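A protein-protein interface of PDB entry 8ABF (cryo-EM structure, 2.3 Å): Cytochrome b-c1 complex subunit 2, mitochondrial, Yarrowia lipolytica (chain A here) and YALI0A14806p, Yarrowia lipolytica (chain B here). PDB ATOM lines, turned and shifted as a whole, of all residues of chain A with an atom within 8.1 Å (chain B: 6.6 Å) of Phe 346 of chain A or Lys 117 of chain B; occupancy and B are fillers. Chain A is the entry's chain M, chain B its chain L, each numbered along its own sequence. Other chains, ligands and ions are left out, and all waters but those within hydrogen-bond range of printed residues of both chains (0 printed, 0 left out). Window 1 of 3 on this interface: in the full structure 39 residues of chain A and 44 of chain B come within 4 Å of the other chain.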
ATOM      1  N   SER A 261      38.167 -20.404  20.590  1.00  0.00           N
ATOM      2  CA  SER A 261      37.062 -20.321  21.537  1.00  0.00           C
ATOM      3  C   SER A 261      37.023 -18.949  22.203  1.00  0.00           C
ATOM      4  O   SER A 261      35.944 -18.377  22.317  1.00  0.00           O
ATOM      5  CB  SER A 261      37.062 -21.446  22.530  1.00  0.00           C
ATOM      6  OG  SER A 261      38.389 -21.835  22.816  1.00  0.00           O
ATOM      7  N   SER A 268      26.095 -17.240  23.449  1.00  0.00           N
ATOM      8  CA  SER A 268      25.960 -18.373  24.344  1.00  0.00           C
ATOM      9  C   SER A 268      24.626 -18.296  25.079  1.00  0.00           C
ATOM     10  O   SER A 268      24.414 -19.029  26.047  1.00  0.00           O
ATOM     11  CB  SER A 268      27.138 -18.467  25.277  1.00  0.00           C
ATOM     12  OG  SER A 268      27.407 -17.206  25.867  1.00  0.00           O
ATOM     13  N   ARG A 339      38.195 -17.746  30.709  1.00  0.00           N
ATOM     14  CA  ARG A 339      37.032 -17.911  29.858  1.00  0.00           C
ATOM     15  C   ARG A 339      37.401 -18.769  28.646  1.00  0.00           C
ATOM     16  O   ARG A 339      36.563 -19.532  28.170  1.00  0.00           O
ATOM     17  CB  ARG A 339      36.488 -16.527  29.528  1.00  0.00           C
ATOM     18  CG  ARG A 339      35.445 -16.473  28.427  1.00  0.00           C
ATOM     19  CD  ARG A 339      34.646 -15.190  28.468  1.00  0.00           C
ATOM     20  NE  ARG A 339      35.195 -13.995  29.098  1.00  0.00           N
ATOM     21  CZ  ARG A 339      35.343 -12.812  28.517  1.00  0.00           C
ATOM     22  NH1 ARG A 339      34.973 -12.622  27.261  1.00  0.00           N
ATOM     23  NH2 ARG A 339      35.851 -11.809  29.209  1.00  0.00           N
ATOM     24  N   ALA A 340      38.661 -18.695  28.190  1.00  0.00           N
ATOM     25  CA  ALA A 340      39.024 -19.422  26.983  1.00  0.00           C
ATOM     26  C   ALA A 340      39.199 -20.892  27.325  1.00  0.00           C
ATOM     27  O   ALA A 340      38.829 -21.754  26.536  1.00  0.00           O
ATOM     28  CB  ALA A 340      40.266 -18.870  26.333  1.00  0.00           C
ATOM     29  N   TYR A 341      39.744 -21.140  28.515  1.00  0.00           N
ATOM     30  CA  TYR A 341      39.920 -22.496  28.981  1.00  0.00           C
ATOM     31  C   TYR A 341      38.559 -23.162  29.159  1.00  0.00           C
ATOM     32  O   TYR A 341      38.395 -24.334  28.841  1.00  0.00           O
ATOM     33  CB  TYR A 341      40.608 -22.450  30.339  1.00  0.00           C
ATOM     34  CG  TYR A 341      40.655 -23.773  31.048  1.00  0.00           C
ATOM     35  CD1 TYR A 341      41.306 -24.851  30.472  1.00  0.00           C
ATOM     36  CD2 TYR A 341      40.085 -23.940  32.302  1.00  0.00           C
ATOM     37  CE1 TYR A 341      41.391 -26.071  31.119  1.00  0.00           C
ATOM     38  CE2 TYR A 341      40.145 -25.164  32.955  1.00  0.00           C
ATOM     39  CZ  TYR A 341      40.804 -26.229  32.363  1.00  0.00           C
ATOM     40  OH  TYR A 341      40.883 -27.442  32.985  1.00  0.00           O
ATOM     41  N   ALA A 342      37.614 -22.405  29.718  1.00  0.00           N
ATOM     42  CA  ALA A 342      36.287 -22.922  29.990  1.00  0.00           C
ATOM     43  C   ALA A 342      35.568 -23.237  28.685  1.00  0.00           C
ATOM     44  O   ALA A 342      35.011 -24.316  28.551  1.00  0.00           O
ATOM     45  CB  ALA A 342      35.499 -21.940  30.807  1.00  0.00           C
ATOM     46  N   LYS A 343      35.541 -22.274  27.756  1.00  0.00           N
ATOM     47  CA  LYS A 343      34.828 -22.481  26.504  1.00  0.00           C
ATOM     48  C   LYS A 343      35.493 -23.593  25.702  1.00  0.00           C
ATOM     49  O   LYS A 343      34.816 -24.302  24.957  1.00  0.00           O
ATOM     50  CB  LYS A 343      34.743 -21.203  25.671  1.00  0.00           C
ATOM     51  CG  LYS A 343      33.922 -20.092  26.302  1.00  0.00           C
ATOM     52  CD  LYS A 343      33.025 -19.403  25.318  1.00  0.00           C
ATOM     53  CE  LYS A 343      33.695 -18.228  24.645  1.00  0.00           C
ATOM     54  NZ  LYS A 343      32.936 -17.793  23.452  1.00  0.00           N
ATOM     55  N   SER A 344      36.806 -23.774  25.888  1.00  0.00           N
ATOM     56  CA  SER A 344      37.503 -24.774  25.098  1.00  0.00           C
ATOM     57  C   SER A 344      37.291 -26.178  25.661  1.00  0.00           C
ATOM     58  O   SER A 344      37.131 -27.105  24.877  1.00  0.00           O
ATOM     59  CB  SER A 344      38.957 -24.447  24.879  1.00  0.00           C
ATOM     60  OG  SER A 344      39.682 -24.544  26.092  1.00  0.00           O
ATOM     61  N   LYS A 345      37.344 -26.338  26.994  1.00  0.00           N
ATOM     62  CA  LYS A 345      37.058 -27.619  27.627  1.00  0.00           C
ATOM     63  C   LYS A 345      35.652 -28.073  27.247  1.00  0.00           C
ATOM     64  O   LYS A 345      35.436 -29.245  26.969  1.00  0.00           O
ATOM     65  CB  LYS A 345      36.987 -27.467  29.145  1.00  0.00           C
ATOM     66  CG  LYS A 345      38.020 -28.247  29.931  1.00  0.00           C
ATOM     67  CD  LYS A 345      37.491 -28.788  31.237  1.00  0.00           C
ATOM     68  CE  LYS A 345      37.538 -27.778  32.361  1.00  0.00           C
ATOM     69  NZ  LYS A 345      37.702 -28.460  33.662  1.00  0.00           N
ATOM     70  N   PHE A 346      34.694 -27.141  27.280  1.00  0.00           N
ATOM     71  CA  PHE A 346      33.324 -27.460  26.929  1.00  0.00           C
ATOM     72  C   PHE A 346      33.236 -27.944  25.487  1.00  0.00           C
ATOM     73  O   PHE A 346      32.571 -28.941  25.230  1.00  0.00           O
ATOM     74  CB  PHE A 346      32.399 -26.262  27.104  1.00  0.00           C
ATOM     75  CG  PHE A 346      30.964 -26.606  26.814  1.00  0.00           C
ATOM     76  CD1 PHE A 346      30.238 -27.391  27.702  1.00  0.00           C
ATOM     77  CD2 PHE A 346      30.345 -26.180  25.648  1.00  0.00           C
ATOM     78  CE1 PHE A 346      28.913 -27.715  27.446  1.00  0.00           C
ATOM     79  CE2 PHE A 346      29.013 -26.486  25.404  1.00  0.00           C
ATOM     80  CZ  PHE A 346      28.304 -27.266  26.294  1.00  0.00           C
ATOM     81  N   ALA A 347      33.876 -27.231  24.555  1.00  0.00           N
ATOM     82  CA  ALA A 347      33.812 -27.615  23.152  1.00  0.00           C
ATOM     83  C   ALA A 347      34.385 -29.017  22.959  1.00  0.00           C
ATOM     84  O   ALA A 347      33.811 -29.825  22.232  1.00  0.00           O
ATOM     85  CB  ALA A 347      34.525 -26.595  22.299  1.00  0.00           C
ATOM     86  N   ALA A 348      35.486 -29.310  23.664  1.00  0.00           N
ATOM     87  CA  ALA A 348      36.114 -30.617  23.581  1.00  0.00           C
ATOM     88  C   ALA A 348      35.161 -31.700  24.072  1.00  0.00           C
ATOM     89  O   ALA A 348      35.119 -32.773  23.475  1.00  0.00           O
ATOM     90  CB  ALA A 348      37.400 -30.646  24.364  1.00  0.00           C
ATOM     91  N   ALA A 349      34.436 -31.417  25.168  1.00  0.00           N
ATOM     92  CA  ALA A 349      33.610 -32.413  25.838  1.00  0.00           C
ATOM     93  C   ALA A 349      32.461 -32.816  24.929  1.00  0.00           C
ATOM     94  O   ALA A 349      32.274 -33.993  24.662  1.00  0.00           O
ATOM     95  CB  ALA A 349      33.105 -31.910  27.168  1.00  0.00           C
ATOM     96  N   GLU A 350      31.780 -31.817  24.381  1.00  0.00           N
ATOM     97  CA  GLU A 350      30.622 -32.069  23.545  1.00  0.00           C
ATOM     98  C   GLU A 350      31.019 -32.743  22.225  1.00  0.00           C
ATOM     99  O   GLU A 350      30.207 -33.453  21.630  1.00  0.00           O
ATOM    100  CB  GLU A 350      29.808 -30.785  23.411  1.00  0.00           C
ATOM    101  CG  GLU A 350      30.505 -29.732  22.577  1.00  0.00           C
ATOM    102  CD  GLU A 350      29.849 -28.370  22.548  1.00  0.00           C
ATOM    103  OE1 GLU A 350      30.583 -27.379  22.391  1.00  0.00           O
ATOM    104  OE2 GLU A 350      28.607 -28.303  22.642  1.00  0.00           O
ATOM    105  N   ALA A 351      32.262 -32.530  21.766  1.00  0.00           N
ATOM    106  CA  ALA A 351      32.736 -33.172  20.550  1.00  0.00           C
ATOM    107  C   ALA A 351      32.975 -34.661  20.792  1.00  0.00           C
ATOM    108  O   ALA A 351      32.735 -35.482  19.909  1.00  0.00           O
ATOM    109  CB  ALA A 351      33.969 -32.485  20.023  1.00  0.00           C
ATOM    110  N   PHE A 352      33.446 -35.002  21.994  1.00  0.00           N
ATOM    111  CA  PHE A 352      33.682 -36.393  22.335  1.00  0.00           C
ATOM    112  C   PHE A 352      32.357 -37.106  22.618  1.00  0.00           C
ATOM    113  O   PHE A 352      32.302 -38.335  22.606  1.00  0.00           O
ATOM    114  CB  PHE A 352      34.718 -36.498  23.456  1.00  0.00           C
ATOM    115  CG  PHE A 352      35.251 -37.888  23.680  1.00  0.00           C
ATOM    116  CD1 PHE A 352      35.852 -38.593  22.646  1.00  0.00           C
ATOM    117  CD2 PHE A 352      35.148 -38.499  24.924  1.00  0.00           C
ATOM    118  CE1 PHE A 352      36.320 -39.888  22.842  1.00  0.00           C
ATOM    119  CE2 PHE A 352      35.620 -39.789  25.121  1.00  0.00           C
ATOM    120  CZ  PHE A 352      36.201 -40.484  24.080  1.00  0.00           C
ATOM    121  N   GLU A 353      31.285 -36.331  22.827  1.00  0.00           N
ATOM    122  CA  GLU A 353      29.971 -36.893  23.109  1.00  0.00           C
ATOM    123  C   GLU A 353      29.215 -37.176  21.813  1.00  0.00           C
ATOM    124  O   GLU A 353      28.721 -38.290  21.636  1.00  0.00           O
ATOM    125  CB  GLU A 353      29.185 -35.998  24.065  1.00  0.00           C
ATOM    126  CG  GLU A 353      29.628 -36.136  25.512  1.00  0.00           C
ATOM    127  CD  GLU A 353      29.747 -34.824  26.278  1.00  0.00           C
ATOM    128  OE1 GLU A 353      28.989 -33.889  25.962  1.00  0.00           O
ATOM    129  OE2 GLU A 353      30.634 -34.721  27.161  1.00  0.00           O
ATOM    130  N   ASN A 354      29.153 -36.183  20.908  1.00  0.00           N
ATOM    131  CA  ASN A 354      28.495 -36.316  19.616  1.00  0.00           C
ATOM    132  C   ASN A 354      29.068 -37.523  18.868  1.00  0.00           C
ATOM    133  O   ASN A 354      30.265 -37.543  18.582  1.00  0.00           O
ATOM    134  CB  ASN A 354      28.615 -35.042  18.777  1.00  0.00           C
ATOM    135  CG  ASN A 354      28.135 -35.214  17.346  1.00  0.00           C
ATOM    136  OD1 ASN A 354      27.054 -35.731  17.071  1.00  0.00           O
ATOM    137  ND2 ASN A 354      28.952 -34.794  16.413  1.00  0.00           N
ATOM    138  N   PRO A 375      38.756 -34.343  27.260  1.00  0.00           N
ATOM    139  CA  PRO A 375      38.286 -33.014  27.661  1.00  0.00           C
ATOM    140  C   PRO A 375      38.744 -32.565  29.045  1.00  0.00           C
ATOM    141  O   PRO A 375      38.933 -31.376  29.272  1.00  0.00           O
ATOM    142  CB  PRO A 375      36.756 -33.120  27.623  1.00  0.00           C
ATOM    143  CG  PRO A 375      36.462 -34.597  27.446  1.00  0.00           C
ATOM    144  CD  PRO A 375      37.665 -35.170  26.730  1.00  0.00           C
ATOM    145  N   VAL A 378      42.461 -31.029  28.736  1.00  0.00           N
ATOM    146  CA  VAL A 378      42.625 -29.835  27.934  1.00  0.00           C
ATOM    147  C   VAL A 378      43.463 -28.838  28.727  1.00  0.00           C
ATOM    148  O   VAL A 378      43.149 -28.533  29.876  1.00  0.00           O
ATOM    149  CB  VAL A 378      41.227 -29.307  27.566  1.00  0.00           C
ATOM    150  CG1 VAL A 378      41.187 -27.829  27.226  1.00  0.00           C
ATOM    151  CG2 VAL A 378      40.612 -30.139  26.457  1.00  0.00           C
ATOM    152  N   THR B  51      29.438 -33.738  30.441  1.00  0.00           N
ATOM    153  CA  THR B  51      28.661 -32.525  30.271  1.00  0.00           C
ATOM    154  C   THR B  51      27.260 -32.789  30.820  1.00  0.00           C
ATOM    155  O   THR B  51      26.812 -33.932  30.802  1.00  0.00           O
ATOM    156  CB  THR B  51      28.744 -32.151  28.786  1.00  0.00           C
ATOM    157  OG1 THR B  51      29.718 -31.113  28.680  1.00  0.00           O
ATOM    158  CG2 THR B  51      27.422 -31.783  28.156  1.00  0.00           C
ATOM    159  N   ALA B  52      26.562 -31.744  31.286  1.00  0.00           N
ATOM    160  CA  ALA B  52      25.234 -31.905  31.862  1.00  0.00           C
ATOM    161  C   ALA B  52      24.276 -30.877  31.277  1.00  0.00           C
ATOM    162  O   ALA B  52      24.686 -29.770  30.984  1.00  0.00           O
ATOM    163  CB  ALA B  52      25.329 -31.722  33.344  1.00  0.00           C
ATOM    164  N   THR B  53      23.010 -31.260  31.106  1.00  0.00           N
ATOM    165  CA  THR B  53      21.963 -30.320  30.749  1.00  0.00           C
ATOM    166  C   THR B  53      20.992 -30.199  31.921  1.00  0.00           C
ATOM    167  O   THR B  53      20.267 -31.143  32.188  1.00  0.00           O
ATOM    168  CB  THR B  53      21.232 -30.786  29.481  1.00  0.00           C
ATOM    169  OG1 THR B  53      22.230 -30.899  28.463  1.00  0.00           O
ATOM    170  CG2 THR B  53      20.148 -29.820  29.061  1.00  0.00           C
ATOM    171  N   VAL B  54      20.986 -29.058  32.617  1.00  0.00           N
ATOM    172  CA  VAL B  54      19.960 -28.769  33.606  1.00  0.00           C
ATOM    173  C   VAL B  54      19.040 -27.700  33.037  1.00  0.00           C
ATOM    174  O   VAL B  54      19.478 -26.781  32.345  1.00  0.00           O
ATOM    175  CB  VAL B  54      20.550 -28.312  34.951  1.00  0.00           C
ATOM    176  CG1 VAL B  54      21.447 -29.379  35.544  1.00  0.00           C
ATOM    177  CG2 VAL B  54      21.301 -27.000  34.807  1.00  0.00           C
ATOM    178  N   MET B  99      31.111 -19.520  32.347  1.00  0.00           N
ATOM    179  CA  MET B  99      30.733 -20.896  32.631  1.00  0.00           C
ATOM    180  C   MET B  99      31.423 -21.814  31.632  1.00  0.00           C
ATOM    181  O   MET B  99      32.010 -22.833  32.009  1.00  0.00           O
ATOM    182  CB  MET B  99      29.250 -21.123  32.356  1.00  0.00           C
ATOM    183  CG  MET B  99      28.324 -21.143  33.512  1.00  0.00           C
ATOM    184  SD  MET B  99      26.931 -22.251  33.053  1.00  0.00           S
ATOM    185  CE  MET B  99      26.776 -22.007  31.277  1.00  0.00           C
ATOM    186  N   GLY B 100      31.302 -21.461  30.348  1.00  0.00           N
ATOM    187  CA  GLY B 100      31.856 -22.320  29.319  1.00  0.00           C
ATOM    188  C   GLY B 100      30.801 -22.882  28.374  1.00  0.00           C
ATOM    189  O   GLY B 100      31.073 -23.055  27.186  1.00  0.00           O
ATOM    190  N   GLY B 101      29.609 -23.169  28.905  1.00  0.00           N
ATOM    191  CA  GLY B 101      28.544 -23.742  28.103  1.00  0.00           C
ATOM    192  C   GLY B 101      27.635 -22.645  27.568  1.00  0.00           C
ATOM    193  O   GLY B 101      28.073 -21.515  27.392  1.00  0.00           O
ATOM    194  N   HIS B 102      26.369 -22.989  27.334  1.00  0.00           N
ATOM    195  CA  HIS B 102      25.413 -22.019  26.830  1.00  0.00           C
ATOM    196  C   HIS B 102      24.073 -22.187  27.537  1.00  0.00           C
ATOM    197  O   HIS B 102      23.840 -23.177  28.227  1.00  0.00           O
ATOM    198  CB  HIS B 102      25.276 -22.169  25.312  1.00  0.00           C
ATOM    199  CG  HIS B 102      24.854 -23.541  24.915  1.00  0.00           C
ATOM    200  ND1 HIS B 102      25.763 -24.559  24.709  1.00  0.00           N
ATOM    201  CD2 HIS B 102      23.631 -24.070  24.709  1.00  0.00           C
ATOM    202  CE1 HIS B 102      25.119 -25.659  24.392  1.00  0.00           C
ATOM    203  NE2 HIS B 102      23.809 -25.382  24.365  1.00  0.00           N
ATOM    204  N   LEU B 103      23.198 -21.208  27.309  1.00  0.00           N
ATOM    205  CA  LEU B 103      21.825 -21.234  27.773  1.00  0.00           C
ATOM    206  C   LEU B 103      20.929 -21.245  26.552  1.00  0.00           C
ATOM    207  O   LEU B 103      21.327 -20.769  25.493  1.00  0.00           O
ATOM    208  CB  LEU B 103      21.576 -19.963  28.576  1.00  0.00           C
ATOM    209  CG  LEU B 103      21.614 -20.117  30.087  1.00  0.00           C
ATOM    210  CD1 LEU B 103      23.010 -20.488  30.586  1.00  0.00           C
ATOM    211  CD2 LEU B 103      21.168 -18.814  30.703  1.00  0.00           C
ATOM    212  N   ASN B 104      19.730 -21.808  26.692  1.00  0.00           N
ATOM    213  CA  ASN B 104      18.805 -21.845  25.580  1.00  0.00           C
ATOM    214  C   ASN B 104      17.384 -21.822  26.120  1.00  0.00           C
ATOM    215  O   ASN B 104      17.167 -22.188  27.272  1.00  0.00           O
ATOM    216  CB  ASN B 104      19.046 -23.079  24.721  1.00  0.00           C
ATOM    217  CG  ASN B 104      18.368 -22.959  23.382  1.00  0.00           C
ATOM    218  OD1 ASN B 104      18.227 -21.868  22.834  1.00  0.00           O
ATOM    219  ND2 ASN B 104      17.938 -24.088  22.852  1.00  0.00           N
ATOM    220  N   TYR B 115      16.996 -23.863  29.545  1.00  0.00           N
ATOM    221  CA  TYR B 115      17.976 -24.818  30.028  1.00  0.00           C
ATOM    222  C   TYR B 115      19.392 -24.308  29.829  1.00  0.00           C
ATOM    223  O   TYR B 115      19.640 -23.390  29.058  1.00  0.00           O
ATOM    224  CB  TYR B 115      17.780 -26.209  29.421  1.00  0.00           C
ATOM    225  CG  TYR B 115      18.066 -26.318  27.951  1.00  0.00           C
ATOM    226  CD1 TYR B 115      19.342 -26.600  27.488  1.00  0.00           C
ATOM    227  CD2 TYR B 115      17.048 -26.167  27.025  1.00  0.00           C
ATOM    228  CE1 TYR B 115      19.599 -26.722  26.132  1.00  0.00           C
ATOM    229  CE2 TYR B 115      17.290 -26.266  25.664  1.00  0.00           C
ATOM    230  CZ  TYR B 115      18.568 -26.562  25.222  1.00  0.00           C
ATOM    231  OH  TYR B 115      18.811 -26.660  23.886  1.00  0.00           O
ATOM    232  N   ALA B 116      20.317 -24.992  30.488  1.00  0.00           N
ATOM    233  CA  ALA B 116      21.720 -24.642  30.440  1.00  0.00           C
ATOM    234  C   ALA B 116      22.508 -25.918  30.208  1.00  0.00           C
ATOM    235  O   ALA B 116      22.379 -26.861  30.982  1.00  0.00           O
ATOM    236  CB  ALA B 116      22.111 -24.052  31.760  1.00  0.00           C
ATOM    237  N   LYS B 117      23.332 -25.927  29.160  1.00  0.00           N
ATOM    238  CA  LYS B 117      24.274 -27.018  28.985  1.00  0.00           C
ATOM    239  C   LYS B 117      25.627 -26.546  29.491  1.00  0.00           C
ATOM    240  O   LYS B 117      26.051 -25.445  29.158  1.00  0.00           O
ATOM    241  CB  LYS B 117      24.342 -27.463  27.524  1.00  0.00           C
ATOM    242  CG  LYS B 117      24.857 -28.870  27.309  1.00  0.00           C
ATOM    243  CD  LYS B 117      24.726 -29.254  25.851  1.00  0.00           C
ATOM    244  CE  LYS B 117      25.502 -30.481  25.434  1.00  0.00           C
ATOM    245  NZ  LYS B 117      24.772 -31.742  25.716  1.00  0.00           N
ATOM    246  N   SER B 118      26.277 -27.368  30.313  1.00  0.00           N
ATOM    247  CA  SER B 118      27.551 -26.962  30.877  1.00  0.00           C
ATOM    248  C   SER B 118      28.469 -28.167  31.026  1.00  0.00           C
ATOM    249  O   SER B 118      28.182 -29.251  30.518  1.00  0.00           O
ATOM    250  CB  SER B 118      27.360 -26.251  32.198  1.00  0.00           C
ATOM    251  OG  SER B 118      26.709 -27.115  33.110  1.00  0.00           O
ATOM    252  N   PHE B 119      29.591 -27.921  31.710  1.00  0.00           N
ATOM    253  CA  PHE B 119      30.500 -28.934  32.204  1.00  0.00           C
ATOM    254  C   PHE B 119      29.925 -29.517  33.492  1.00  0.00           C
ATOM    255  O   PHE B 119      29.036 -28.926  34.103  1.00  0.00           O
ATOM    256  CB  PHE B 119      31.915 -28.351  32.342  1.00  0.00           C
ATOM    257  CG  PHE B 119      32.943 -29.392  32.007  1.00  0.00           C
ATOM    258  CD1 PHE B 119      33.132 -29.764  30.684  1.00  0.00           C
ATOM    259  CD2 PHE B 119      33.592 -30.111  33.002  1.00  0.00           C
ATOM    260  CE1 PHE B 119      33.997 -30.797  30.363  1.00  0.00           C
ATOM    261  CE2 PHE B 119      34.451 -31.154  32.677  1.00  0.00           C
ATOM    262  CZ  PHE B 119      34.649 -31.490  31.358  1.00  0.00           C
ATOM    263  N   SER B 126      25.007 -22.747  36.723  1.00  0.00           N
ATOM    264  CA  SER B 126      23.946 -22.717  35.740  1.00  0.00           C
ATOM    265  C   SER B 126      22.569 -22.758  36.405  1.00  0.00           C
ATOM    266  O   SER B 126      21.663 -22.025  35.988  1.00  0.00           O
ATOM    267  CB  SER B 126      24.160 -23.787  34.713  1.00  0.00           C
ATOM    268  OG  SER B 126      24.453 -25.027  35.327  1.00  0.00           O
ATOM    269  N   GLY B 399      21.948 -37.585  23.084  1.00  0.00           N
ATOM    270  CA  GLY B 399      22.741 -36.751  23.968  1.00  0.00           C
ATOM    271  C   GLY B 399      21.924 -36.286  25.168  1.00  0.00           C
ATOM    272  O   GLY B 399      20.738 -36.588  25.279  1.00  0.00           O
ATOM    273  N   THR B 400      22.586 -35.545  26.060  1.00  0.00           N
ATOM    274  CA  THR B 400      21.999 -35.154  27.330  1.00  0.00           C
ATOM    275  C   THR B 400      20.822 -34.212  27.109  1.00  0.00           C
ATOM    276  O   THR B 400      19.883 -34.216  27.890  1.00  0.00           O
ATOM    277  CB  THR B 400      23.042 -34.520  28.256  1.00  0.00           C
ATOM    278  OG1 THR B 400      23.432 -33.271  27.697  1.00  0.00           O
ATOM    279  CG2 THR B 400      24.262 -35.387  28.455  1.00  0.00           C
ATOM    280  N   THR B 401      20.874 -33.411  26.044  1.00  0.00           N
ATOM    281  CA  THR B 401      19.808 -32.456  25.818  1.00  0.00           C
ATOM    282  C   THR B 401      18.546 -33.194  25.389  1.00  0.00           C
ATOM    283  O   THR B 401      17.462 -32.770  25.755  1.00  0.00           O
ATOM    284  CB  THR B 401      20.215 -31.339  24.853  1.00  0.00           C
ATOM    285  OG1 THR B 401      21.366 -30.720  25.419  1.00  0.00           O
ATOM    286  CG2 THR B 401      19.142 -30.284  24.681  1.00  0.00           C
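The backbone NH of Leu 103 of chain B sits at hydrogen-bond distance from the backbone carbonyl oxygen of Ser 268 of chain A, 2.8 Å away.
The side-chain hydroxyl (OG1) of Thr 51 of chain B is in hydrogen-bond range of the backbone carbonyl oxygen (O) of Ser 118 of chain B, 3.0 Å away. OH of Tyr 341 of chain A lies within hydrogen-bond range of NZ of Lys 345 of chain A, at 3.4 Å. NZ of Lys 343 of chain A lies close to O of Ser 261 of chain A (3.3 Å). The backbone carbonyl oxygen (O) of Ala 52 of chain B lies within hydrogen-bond range of the backbone NH (N) of Ser 118 of chain B (3.0 Å). OG1 of Thr 400 of chain B is in hydrogen-bond range of NZ of Lys 117 of chain B (2.8 Å). N of Lys 117 of chain B sits at hydrogen-bond distance from O of His 102 of chain B.
Among the printed residues, pairs that only touch across the chains: Ser 268 of chain A with His 102 of chain B (3.2 Å), Glu 353 of chain A with Thr 51 of chain B (3.3 Å), Phe 346 of chain A with Gly 100 of chain B (3.5 Å), Ala 349 of chain A with Phe 119 of chain B (3.5 Å), Phe 346 of chain A with Ser 118 of chain B (3.5 Å), Phe 346 of chain A with Thr 51 of chain B (3.7 Å), Ala 349 of chain A with Thr 51 of chain B (3.8 Å), Ala 342 of chain A with Met 99 of chain B (3.8 Å), Ala 342 of chain A with Gly 100 of chain B (3.8 Å), Ser 268 of chain A with Gly 101 of chain B (3.8 Å), Phe 346 of chain A with His 102 of chain B (3.8 Å), Lys 343 of chain A with Gly 100 of chain B (3.9 Å), Phe 346 of chain A with Gly 101 of chain B (3.9 Å), Lys 345 of chain A with Phe 119 of chain B (3.9 Å) and Phe 346 of chain A with Lys 117 of chain B (3.9 Å).
Phe 346 of chain A touches just these residues of chain B: Thr 51, Gly 100, Gly 101, His 102, Lys 117 and Ser 118. Of chain A, only Phe 346 comes within 4 Å of Lys 117 of chain B. Ala 116 of chain B touches none of the printed residues of chain A. Of the printed residues of chain A, Phe 119 of chain B touches Lys 345 (3.9 Å) and Ala 349 (3.5 Å). Of the printed residues of chain A, Gly 101 of chain B touches Ser 268 and Phe 346. Of the printed residues of chain A, Leu 103 of chain B touches Ser 268. The nearest printed residue of chain A that does not touch Phe 119 of chain B is Phe 346 of chain A (4.1 Å).
Printed residues of chain A that touch a printed residue of chain B: Ser 268, Ala 342, Lys 343, Lys 345, Phe 346, Ala 349 and Glu 353. Hydrophobic or aromatic side chains of chain A that line the printed part of chain B: Ala 342, Phe 346 and Ala 349. Of the 19 printed residues of chain B, 9 touch a printed residue of chain A. Printed residues of chain B that touch a printed residue of chain A: Thr 51, Met 99, Gly 100, Gly 101, His 102, Leu 103, Lys 117, Ser 118 and Phe 119. Along chain B the printed residues that touch a printed residue of chain A span positions 51 to 119. Among the printed residues, 16 pairs touch across the chains. Among the printed residues, no Asp or Glu carboxylate lies within 4 Å of a Lys or Arg side-chain nitrogen of the other chain.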
